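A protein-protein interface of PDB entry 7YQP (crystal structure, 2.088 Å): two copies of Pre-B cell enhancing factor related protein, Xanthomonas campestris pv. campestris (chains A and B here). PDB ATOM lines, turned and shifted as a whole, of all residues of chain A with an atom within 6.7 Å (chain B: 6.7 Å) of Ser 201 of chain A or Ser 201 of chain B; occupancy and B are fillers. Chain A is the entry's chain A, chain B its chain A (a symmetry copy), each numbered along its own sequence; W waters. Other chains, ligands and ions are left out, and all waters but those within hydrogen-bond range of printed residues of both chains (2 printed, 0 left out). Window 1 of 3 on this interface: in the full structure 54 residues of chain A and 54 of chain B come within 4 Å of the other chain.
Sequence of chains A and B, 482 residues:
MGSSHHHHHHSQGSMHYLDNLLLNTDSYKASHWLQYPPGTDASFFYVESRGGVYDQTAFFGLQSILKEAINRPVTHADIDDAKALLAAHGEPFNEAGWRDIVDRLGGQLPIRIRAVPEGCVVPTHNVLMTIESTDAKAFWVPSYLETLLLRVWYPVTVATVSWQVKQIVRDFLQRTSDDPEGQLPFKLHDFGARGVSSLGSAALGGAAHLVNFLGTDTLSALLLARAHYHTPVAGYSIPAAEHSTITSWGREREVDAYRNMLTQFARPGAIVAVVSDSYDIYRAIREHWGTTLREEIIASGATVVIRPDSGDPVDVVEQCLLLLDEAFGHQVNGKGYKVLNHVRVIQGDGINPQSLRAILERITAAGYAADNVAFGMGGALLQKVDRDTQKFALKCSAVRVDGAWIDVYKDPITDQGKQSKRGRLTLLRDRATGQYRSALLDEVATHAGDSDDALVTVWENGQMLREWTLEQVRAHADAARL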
ATOM      1  N   TYR A 154     -13.603 -29.398  17.171  1.00  0.00           N
ATOM      2  CA  TYR A 154     -14.820 -29.789  17.869  1.00  0.00           C
ATOM      3  C   TYR A 154     -15.747 -30.611  16.976  1.00  0.00           C
ATOM      4  O   TYR A 154     -16.128 -31.721  17.367  1.00  0.00           O
ATOM      5  CB  TYR A 154     -15.535 -28.557  18.432  1.00  0.00           C
ATOM      6  CG  TYR A 154     -16.874 -28.891  19.039  1.00  0.00           C
ATOM      7  CD1 TYR A 154     -16.964 -29.729  20.143  1.00  0.00           C
ATOM      8  CD2 TYR A 154     -18.050 -28.384  18.501  1.00  0.00           C
ATOM      9  CE1 TYR A 154     -18.187 -30.046  20.698  1.00  0.00           C
ATOM     10  CE2 TYR A 154     -19.277 -28.697  19.048  1.00  0.00           C
ATOM     11  CZ  TYR A 154     -19.341 -29.529  20.146  1.00  0.00           C
ATOM     12  OH  TYR A 154     -20.565 -29.841  20.698  1.00  0.00           O
ATOM     13  N   VAL A 196     -24.720 -29.133  26.372  1.00  0.00           N
ATOM     14  CA  VAL A 196     -23.674 -28.521  25.580  1.00  0.00           C
ATOM     15  C   VAL A 196     -23.554 -27.063  26.003  1.00  0.00           C
ATOM     16  O   VAL A 196     -24.470 -26.481  26.588  1.00  0.00           O
ATOM     17  CB  VAL A 196     -23.955 -28.665  24.069  1.00  0.00           C
ATOM     18  CG1 VAL A 196     -25.051 -27.707  23.645  1.00  0.00           C
ATOM     19  CG2 VAL A 196     -22.679 -28.460  23.262  1.00  0.00           C
ATOM     20  N   SER A 197     -22.402 -26.460  25.708  1.00  0.00           N
ATOM     21  CA  SER A 197     -22.058 -25.155  26.257  1.00  0.00           C
ATOM     22  C   SER A 197     -22.753 -23.985  25.569  1.00  0.00           C
ATOM     23  O   SER A 197     -22.855 -22.915  26.174  1.00  0.00           O
ATOM     24  CB  SER A 197     -20.541 -24.978  26.209  1.00  0.00           C
ATOM     25  OG  SER A 197     -20.125 -24.601  24.912  1.00  0.00           O
ATOM     26  N   SER A 198     -23.232 -24.143  24.336  1.00  0.00           N
ATOM     27  CA  SER A 198     -23.896 -23.032  23.662  1.00  0.00           C
ATOM     28  C   SER A 198     -24.776 -23.558  22.540  1.00  0.00           C
ATOM     29  O   SER A 198     -24.594 -24.676  22.051  1.00  0.00           O
ATOM     30  CB  SER A 198     -22.885 -22.023  23.103  1.00  0.00           C
ATOM     31  N   LEU A 199     -25.735 -22.719  22.139  1.00  0.00           N
ATOM     32  CA  LEU A 199     -26.590 -23.031  21.001  1.00  0.00           C
ATOM     33  C   LEU A 199     -25.769 -23.330  19.753  1.00  0.00           C
ATOM     34  O   LEU A 199     -26.072 -24.271  19.010  1.00  0.00           O
ATOM     35  CB  LEU A 199     -27.548 -21.867  20.743  1.00  0.00           C
ATOM     36  CG  LEU A 199     -28.365 -21.907  19.448  1.00  0.00           C
ATOM     37  CD1 LEU A 199     -29.285 -23.108  19.431  1.00  0.00           C
ATOM     38  CD2 LEU A 199     -29.163 -20.621  19.271  1.00  0.00           C
ATOM     39  N   GLY A 200     -24.722 -22.536  19.508  1.00  0.00           N
ATOM     40  CA  GLY A 200     -23.894 -22.763  18.334  1.00  0.00           C
ATOM     41  C   GLY A 200     -23.147 -24.081  18.398  1.00  0.00           C
ATOM     42  O   GLY A 200     -22.952 -24.748  17.378  1.00  0.00           O
ATOM     43  N   SER A 201     -22.706 -24.467  19.598  1.00  0.00           N
ATOM     44  CA  SER A 201     -22.100 -25.782  19.780  1.00  0.00           C
ATOM     45  C   SER A 201     -23.131 -26.895  19.656  1.00  0.00           C
ATOM     46  O   SER A 201     -22.813 -27.980  19.153  1.00  0.00           O
ATOM     47  CB  SER A 201     -21.406 -25.857  21.139  1.00  0.00           C
ATOM     48  OG  SER A 201     -20.476 -24.801  21.301  1.00  0.00           O
ATOM     49  N   ALA A 202     -24.363 -26.650  20.118  1.00  0.00           N
ATOM     50  CA  ALA A 202     -25.433 -27.624  19.925  1.00  0.00           C
ATOM     51  C   ALA A 202     -25.693 -27.865  18.445  1.00  0.00           C
ATOM     52  O   ALA A 202     -25.919 -29.005  18.019  1.00  0.00           O
ATOM     53  CB  ALA A 202     -26.711 -27.146  20.611  1.00  0.00           C
ATOM     54  N   ALA A 203     -25.666 -26.799  17.644  1.00  0.00           N
ATOM     55  CA  ALA A 203     -25.921 -26.937  16.216  1.00  0.00           C
ATOM     56  C   ALA A 203     -24.772 -27.657  15.522  1.00  0.00           C
ATOM     57  O   ALA A 203     -24.980 -28.662  14.834  1.00  0.00           O
ATOM     58  CB  ALA A 203     -26.152 -25.559  15.593  1.00  0.00           C
ATOM     59  N   LEU A 204     -23.546 -27.161  15.704  1.00  0.00           N
ATOM     60  CA  LEU A 204     -22.398 -27.721  14.997  1.00  0.00           C
ATOM     61  C   LEU A 204     -22.092 -29.134  15.473  1.00  0.00           C
ATOM     62  O   LEU A 204     -21.937 -30.052  14.660  1.00  0.00           O
ATOM     63  CB  LEU A 204     -21.182 -26.812  15.182  1.00  0.00           C
ATOM     64  CG  LEU A 204     -19.916 -27.124  14.378  1.00  0.00           C
ATOM     65  CD1 LEU A 204     -20.258 -27.521  12.950  1.00  0.00           C
ATOM     66  CD2 LEU A 204     -18.976 -25.928  14.395  1.00  0.00           C
ATOM     67  N   GLY A 205     -21.992 -29.330  16.787  1.00  0.00           N
ATOM     68  CA  GLY A 205     -21.699 -30.658  17.301  1.00  0.00           C
ATOM     69  C   GLY A 205     -22.799 -31.659  17.008  1.00  0.00           C
ATOM     70  O   GLY A 205     -22.526 -32.816  16.676  1.00  0.00           O
ATOM     71  N   GLY A 206     -24.057 -31.233  17.130  1.00  0.00           N
ATOM     72  CA  GLY A 206     -25.155 -32.111  16.764  1.00  0.00           C
ATOM     73  C   GLY A 206     -25.102 -32.510  15.304  1.00  0.00           C
ATOM     74  O   GLY A 206     -25.375 -33.660  14.955  1.00  0.00           O
ATOM     75  N   ALA A 207     -24.739 -31.564  14.432  1.00  0.00           N
ATOM     76  CA  ALA A 207     -24.572 -31.885  13.019  1.00  0.00           C
ATOM     77  C   ALA A 207     -23.468 -32.913  12.816  1.00  0.00           C
ATOM     78  O   ALA A 207     -23.577 -33.787  11.948  1.00  0.00           O
ATOM     79  CB  ALA A 207     -24.267 -30.617  12.223  1.00  0.00           C
ATOM     80  N   THR A 218     -31.602 -32.784  18.910  1.00  0.00           N
ATOM     81  CA  THR A 218     -30.997 -31.457  18.857  1.00  0.00           C
ATOM     82  C   THR A 218     -31.522 -30.763  17.610  1.00  0.00           C
ATOM     83  O   THR A 218     -30.942 -30.861  16.525  1.00  0.00           O
ATOM     84  CB  THR A 218     -29.479 -31.553  18.853  1.00  0.00           C
ATOM     85  OG1 THR A 218     -29.053 -32.403  19.926  1.00  0.00           O
ATOM     86  CG2 THR A 218     -28.860 -30.174  19.032  1.00  0.00           C
ATOM     87  N   SER A 220     -31.315 -27.830  16.887  1.00  0.00           N
ATOM     88  CA  SER A 220     -30.297 -26.920  16.384  1.00  0.00           C
ATOM     89  C   SER A 220     -29.464 -27.569  15.286  1.00  0.00           C
ATOM     90  O   SER A 220     -28.992 -26.878  14.379  1.00  0.00           O
ATOM     91  CB  SER A 220     -29.408 -26.469  17.541  1.00  0.00           C
ATOM     92  OG  SER A 220     -30.204 -25.944  18.591  1.00  0.00           O
ATOM     93  N   LEU A 382     -21.558 -34.327  23.011  1.00  0.00           N
ATOM     94  CA  LEU A 382     -21.423 -32.957  22.533  1.00  0.00           C
ATOM     95  C   LEU A 382     -20.499 -32.095  23.377  1.00  0.00           C
ATOM     96  O   LEU A 382     -20.020 -31.064  22.885  1.00  0.00           O
ATOM     97  CB  LEU A 382     -22.796 -32.280  22.479  1.00  0.00           C
ATOM     98  CG  LEU A 382     -23.818 -32.836  21.494  1.00  0.00           C
ATOM     99  CD1 LEU A 382     -24.991 -31.874  21.355  1.00  0.00           C
ATOM    100  CD2 LEU A 382     -23.171 -33.111  20.145  1.00  0.00           C
ATOM    101  N   GLN A 383     -20.250 -32.466  24.627  1.00  0.00           N
ATOM    102  CA  GLN A 383     -19.538 -31.573  25.536  1.00  0.00           C
ATOM    103  C   GLN A 383     -18.293 -32.189  26.152  1.00  0.00           C
ATOM    104  O   GLN A 383     -17.297 -31.484  26.345  1.00  0.00           O
ATOM    105  CB  GLN A 383     -20.485 -31.110  26.653  1.00  0.00           C
ATOM    106  CG  GLN A 383     -19.855 -30.155  27.661  1.00  0.00           C
ATOM    107  CD  GLN A 383     -19.481 -28.817  27.047  1.00  0.00           C
ATOM    108  OE1 GLN A 383     -20.137 -28.343  26.116  1.00  0.00           O
ATOM    109  NE2 GLN A 383     -18.430 -28.194  27.575  1.00  0.00           N
ATOM    110  N   TYR B 154     -23.199 -23.658  32.005  1.00  0.00           N
ATOM    111  CA  TYR B 154     -21.876 -23.431  31.439  1.00  0.00           C
ATOM    112  C   TYR B 154     -21.256 -22.132  31.950  1.00  0.00           C
ATOM    113  O   TYR B 154     -20.138 -22.169  32.479  1.00  0.00           O
ATOM    114  CB  TYR B 154     -21.935 -23.458  29.909  1.00  0.00           C
ATOM    115  CG  TYR B 154     -20.621 -23.086  29.272  1.00  0.00           C
ATOM    116  CD1 TYR B 154     -19.490 -23.868  29.468  1.00  0.00           C
ATOM    117  CD2 TYR B 154     -20.503 -21.945  28.487  1.00  0.00           C
ATOM    118  CE1 TYR B 154     -18.281 -23.529  28.894  1.00  0.00           C
ATOM    119  CE2 TYR B 154     -19.298 -21.597  27.912  1.00  0.00           C
ATOM    120  CZ  TYR B 154     -18.190 -22.391  28.119  1.00  0.00           C
ATOM    121  OH  TYR B 154     -16.986 -22.049  27.543  1.00  0.00           O
ATOM    122  N   VAL B 196     -12.096 -23.901  22.786  1.00  0.00           N
ATOM    123  CA  VAL B 196     -13.501 -23.953  23.130  1.00  0.00           C
ATOM    124  C   VAL B 196     -14.272 -24.398  21.893  1.00  0.00           C
ATOM    125  O   VAL B 196     -13.794 -24.299  20.761  1.00  0.00           O
ATOM    126  CB  VAL B 196     -14.000 -22.594  23.665  1.00  0.00           C
ATOM    127  CG1 VAL B 196     -14.156 -21.605  22.527  1.00  0.00           C
ATOM    128  CG2 VAL B 196     -15.297 -22.767  24.447  1.00  0.00           C
ATOM    129  N   SER B 197     -15.486 -24.904  22.111  1.00  0.00           N
ATOM    130  CA  SER B 197     -16.232 -25.584  21.060  1.00  0.00           C
ATOM    131  C   SER B 197     -16.892 -24.645  20.055  1.00  0.00           C
ATOM    132  O   SER B 197     -17.196 -25.083  18.942  1.00  0.00           O
ATOM    133  CB  SER B 197     -17.275 -26.499  21.700  1.00  0.00           C
ATOM    134  OG  SER B 197     -18.410 -25.756  22.099  1.00  0.00           O
ATOM    135  N   SER B 198     -17.125 -23.379  20.399  1.00  0.00           N
ATOM    136  CA  SER B 198     -17.759 -22.469  19.451  1.00  0.00           C
ATOM    137  C   SER B 198     -17.466 -21.029  19.840  1.00  0.00           C
ATOM    138  O   SER B 198     -17.121 -20.730  20.986  1.00  0.00           O
ATOM    139  CB  SER B 198     -19.275 -22.692  19.379  1.00  0.00           C
ATOM    140  N   LEU B 199     -17.617 -20.140  18.854  1.00  0.00           N
ATOM    141  CA  LEU B 199     -17.481 -18.709  19.094  1.00  0.00           C
ATOM    142  C   LEU B 199     -18.411 -18.240  20.205  1.00  0.00           C
ATOM    143  O   LEU B 199     -18.014 -17.445  21.065  1.00  0.00           O
ATOM    144  CB  LEU B 199     -17.764 -17.942  17.802  1.00  0.00           C
ATOM    145  CG  LEU B 199     -17.899 -16.419  17.907  1.00  0.00           C
ATOM    146  CD1 LEU B 199     -16.606 -15.799  18.390  1.00  0.00           C
ATOM    147  CD2 LEU B 199     -18.313 -15.819  16.569  1.00  0.00           C
ATOM    148  N   GLY B 200     -19.657 -18.725  20.202  1.00  0.00           N
ATOM    149  CA  GLY B 200     -20.599 -18.319  21.233  1.00  0.00           C
ATOM    150  C   GLY B 200     -20.192 -18.800  22.612  1.00  0.00           C
ATOM    151  O   GLY B 200     -20.403 -18.107  23.612  1.00  0.00           O
ATOM    152  N   SER B 201     -19.612 -20.001  22.686  1.00  0.00           N
ATOM    153  CA  SER B 201     -19.063 -20.485  23.948  1.00  0.00           C
ATOM    154  C   SER B 201     -17.812 -19.714  24.346  1.00  0.00           C
ATOM    155  O   SER B 201     -17.577 -19.490  25.540  1.00  0.00           O
ATOM    156  CB  SER B 201     -18.750 -21.978  23.847  1.00  0.00           C
ATOM    157  OG  SER B 201     -19.885 -22.714  23.429  1.00  0.00           O
ATOM    158  N   ALA B 202     -16.996 -19.312  23.365  1.00  0.00           N
ATOM    159  CA  ALA B 202     -15.843 -18.466  23.661  1.00  0.00           C
ATOM    160  C   ALA B 202     -16.280 -17.142  24.272  1.00  0.00           C
ATOM    161  O   ALA B 202     -15.646 -16.637  25.207  1.00  0.00           O
ATOM    162  CB  ALA B 202     -15.033 -18.216  22.390  1.00  0.00           C
ATOM    163  N   ALA B 203     -17.363 -16.563  23.752  1.00  0.00           N
ATOM    164  CA  ALA B 203     -17.840 -15.285  24.266  1.00  0.00           C
ATOM    165  C   ALA B 203     -18.427 -15.442  25.663  1.00  0.00           C
ATOM    166  O   ALA B 203     -18.018 -14.747  26.600  1.00  0.00           O
ATOM    167  CB  ALA B 203     -18.875 -14.693  23.308  1.00  0.00           C
ATOM    168  N   LEU B 204     -19.379 -16.363  25.822  1.00  0.00           N
ATOM    169  CA  LEU B 204     -20.071 -16.513  27.099  1.00  0.00           C
ATOM    170  C   LEU B 204     -19.133 -17.036  28.178  1.00  0.00           C
ATOM    171  O   LEU B 204     -19.060 -16.473  29.275  1.00  0.00           O
ATOM    172  CB  LEU B 204     -21.274 -17.442  26.931  1.00  0.00           C
ATOM    173  CG  LEU B 204     -22.240 -17.597  28.109  1.00  0.00           C
ATOM    174  CD1 LEU B 204     -22.504 -16.258  28.781  1.00  0.00           C
ATOM    175  CD2 LEU B 204     -23.542 -18.231  27.641  1.00  0.00           C
ATOM    176  N   GLY B 205     -18.411 -18.119  27.890  1.00  0.00           N
ATOM    177  CA  GLY B 205     -17.500 -18.667  28.881  1.00  0.00           C
ATOM    178  C   GLY B 205     -16.363 -17.723  29.220  1.00  0.00           C
ATOM    179  O   GLY B 205     -15.970 -17.603  30.383  1.00  0.00           O
ATOM    180  N   GLY B 206     -15.814 -17.045  28.211  1.00  0.00           N
ATOM    181  CA  GLY B 206     -14.793 -16.049  28.483  1.00  0.00           C
ATOM    182  C   GLY B 206     -15.307 -14.931  29.366  1.00  0.00           C
ATOM    183  O   GLY B 206     -14.600 -14.457  30.257  1.00  0.00           O
ATOM    184  N   ALA B 207     -16.552 -14.504  29.136  1.00  0.00           N
ATOM    185  CA  ALA B 207     -17.160 -13.496  29.999  1.00  0.00           C
ATOM    186  C   ALA B 207     -17.281 -13.999  31.429  1.00  0.00           C
ATOM    187  O   ALA B 207     -17.104 -13.230  32.382  1.00  0.00           O
ATOM    188  CB  ALA B 207     -18.534 -13.101  29.459  1.00  0.00           C
ATOM    189  N   THR B 218      -9.436 -13.677  24.974  1.00  0.00           N
ATOM    190  CA  THR B 218     -10.654 -14.050  24.261  1.00  0.00           C
ATOM    191  C   THR B 218     -11.398 -12.769  23.923  1.00  0.00           C
ATOM    192  O   THR B 218     -12.228 -12.281  24.695  1.00  0.00           O
ATOM    193  CB  THR B 218     -11.505 -14.993  25.099  1.00  0.00           C
ATOM    194  OG1 THR B 218     -10.691 -16.073  25.575  1.00  0.00           O
ATOM    195  CG2 THR B 218     -12.647 -15.557  24.266  1.00  0.00           C
ATOM    196  N   SER B 220     -13.717 -12.414  22.007  1.00  0.00           N
ATOM    197  CA  SER B 220     -15.147 -12.684  21.996  1.00  0.00           C
ATOM    198  C   SER B 220     -15.790 -12.329  23.330  1.00  0.00           C
ATOM    199  O   SER B 220     -16.959 -11.935  23.367  1.00  0.00           O
ATOM    200  CB  SER B 220     -15.381 -14.154  21.658  1.00  0.00           C
ATOM    201  OG  SER B 220     -14.705 -14.491  20.456  1.00  0.00           O
ATOM    202  N   LEU B 382     -12.430 -23.109  29.681  1.00  0.00           N
ATOM    203  CA  LEU B 382     -13.606 -22.858  28.859  1.00  0.00           C
ATOM    204  C   LEU B 382     -14.274 -24.118  28.333  1.00  0.00           C
ATOM    205  O   LEU B 382     -15.451 -24.062  27.953  1.00  0.00           O
ATOM    206  CB  LEU B 382     -13.234 -21.978  27.662  1.00  0.00           C
ATOM    207  CG  LEU B 382     -12.768 -20.555  27.951  1.00  0.00           C
ATOM    208  CD1 LEU B 382     -12.737 -19.740  26.664  1.00  0.00           C
ATOM    209  CD2 LEU B 382     -13.660 -19.899  28.994  1.00  0.00           C
ATOM    210  N   GLN B 383     -13.565 -25.239  28.280  1.00  0.00           N
ATOM    211  CA  GLN B 383     -14.093 -26.418  27.601  1.00  0.00           C
ATOM    212  C   GLN B 383     -14.145 -27.660  28.475  1.00  0.00           C
ATOM    213  O   GLN B 383     -15.085 -28.452  28.353  1.00  0.00           O
ATOM    214  CB  GLN B 383     -13.255 -26.711  26.347  1.00  0.00           C
ATOM    215  CG  GLN B 383     -13.724 -27.917  25.541  1.00  0.00           C
ATOM    216  CD  GLN B 383     -15.092 -27.709  24.914  1.00  0.00           C
ATOM    217  OE1 GLN B 383     -15.462 -26.586  24.563  1.00  0.00           O
ATOM    218  NE2 GLN B 383     -15.845 -28.795  24.757  1.00  0.00           N
HETATM  219  O   HOH W   1     -18.826 -28.230  23.844  1.00  0.00           O
HETATM  220  O   HOH W   2     -17.456 -25.634  25.981  1.00  0.00           O
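Among the printed residues, merely in contact across the chains: Tyr 154 of chain A with Ser 197 of chain B, Ser 197 of chain A with Tyr 154 of chain B, Ser 198 of chain A with Ser 201 of chain B and Ser 201 of chain A with Ser 198 of chain B.
Of the 17 printed residues of chain B, 5 touch a printed residue of chain A. Hydrophobic or aromatic side chains of chain B that line the printed part of chain A: Tyr 154. Hydrophobic or aromatic side chains of chain A within 4 Å of the printed part of chain B: Tyr 154.
Tyr 154 of chain A touches Ser 197 of chain B, and with the chains exchanged Ser 197 of chain A touches Tyr 154 of chain B. Ser 197 of chain B touches its own counterpart, Ser 197 of chain A. Ser 197 of chain A touches Ser 201 of chain B, and with the chains exchanged Ser 201 of chain A touches Ser 197 of chain B. Ser 201 of chain B touches its own counterpart, Ser 201 of chain A. Of the 9 pairs that touch across the chains among the printed residues, 9 have their exchanged pair printed and touching as well.
The side-chain hydroxyl (OH) of Tyr 154 of chain B is in hydrogen-bond range of the backbone carbonyl oxygen (O) of Leu 382 of chain B. The backbone NH of Ser 197 of chain B lies within hydrogen-bond range of the side-chain amide oxygen of Gln 383 of chain B, 3.0 Å away. The backbone NH (N) of Ser 197 of chain A sits at hydrogen-bond distance from the side-chain amide oxygen (OE1) of Gln 383 of chain A (3.0 Å). O of Ser 201 of chain B is in hydrogen-bond range of OH of Tyr 154 of chain B (3.3 Å). The side-chain hydroxyl (OH) of Tyr 154 of chain A sits at hydrogen-bond distance from the backbone carbonyl oxygen (O) of Leu 382 of chain A, at 2.6 Å. O of Ser 201 of chain A sits at hydrogen-bond distance from OH of Tyr 154 of chain A, at 3.3 Å.
Water W1 lies within hydrogen-bond range of the side-chain amide oxygen (OE1) of Gln 383 of chain A (2.6 Å), the side-chain hydroxyl (OG) of Ser 197 of chain B (3.1 Å), the side-chain amide nitrogen (NE2) of Gln 383 of chain B (3.2 Å) and the backbone carbonyl oxygen (O) of Leu 382 of chain A (3.2 Å). Water W2 lies within hydrogen-bond range of OE1 of Gln 383 of chain B (2.6 Å), OG of Ser 197 of chain A (3.1 Å), NE2 of Gln 383 of chain A (3.2 Å) and O of Leu 382 of chain B (3.2 Å).
Printed residues of chain B within 4 Å of Tyr 154 of chain A: Ser 197. Of chain B, only Ser 197 (2.4 Å), Ser 198 (3.1 Å) and Ser 201 (3.0 Å) come within 4 Å of Ser 201 of chain A. Ala 202 of chain A touches none of the printed residues of chain B. Leu 382 of chain A touches none of the printed residues of chain B. Printed residues of chain B within 4 Å of Gln 383 of chain A: Gln 383 (3.4 Å). Ser 201 of chain B touches three residues of chain A. The nearest residue of chain A that does not touch Ser 201 of chain B is Leu 199 of chain A (6.0 Å).
The side-chain hydroxyl (OG) of Ser 197 of chain A lies within hydrogen-bond range of the side-chain hydroxyl (OG) of Ser 201 of chain B. The backbone carbonyl oxygen (O) of Gln 383 of chain A is in hydrogen-bond range of the side-chain amide nitrogen (NE2) of Gln 383 of chain B (3.4 Å). The side-chain hydroxyl of Ser 201 of chain A is in hydrogen-bond range of the side-chain hydroxyl of Ser 197 of chain B (2.4 Å). The side-chain hydroxyl (OG) of Ser 201 of chain A is in hydrogen-bond range of the side-chain hydroxyl (OG) of Ser 201 of chain B, 3.0 Å away. OG of Ser 197 of chain A lies within hydrogen-bond range of OG of Ser 197 of chain B, 3.5 Å away.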
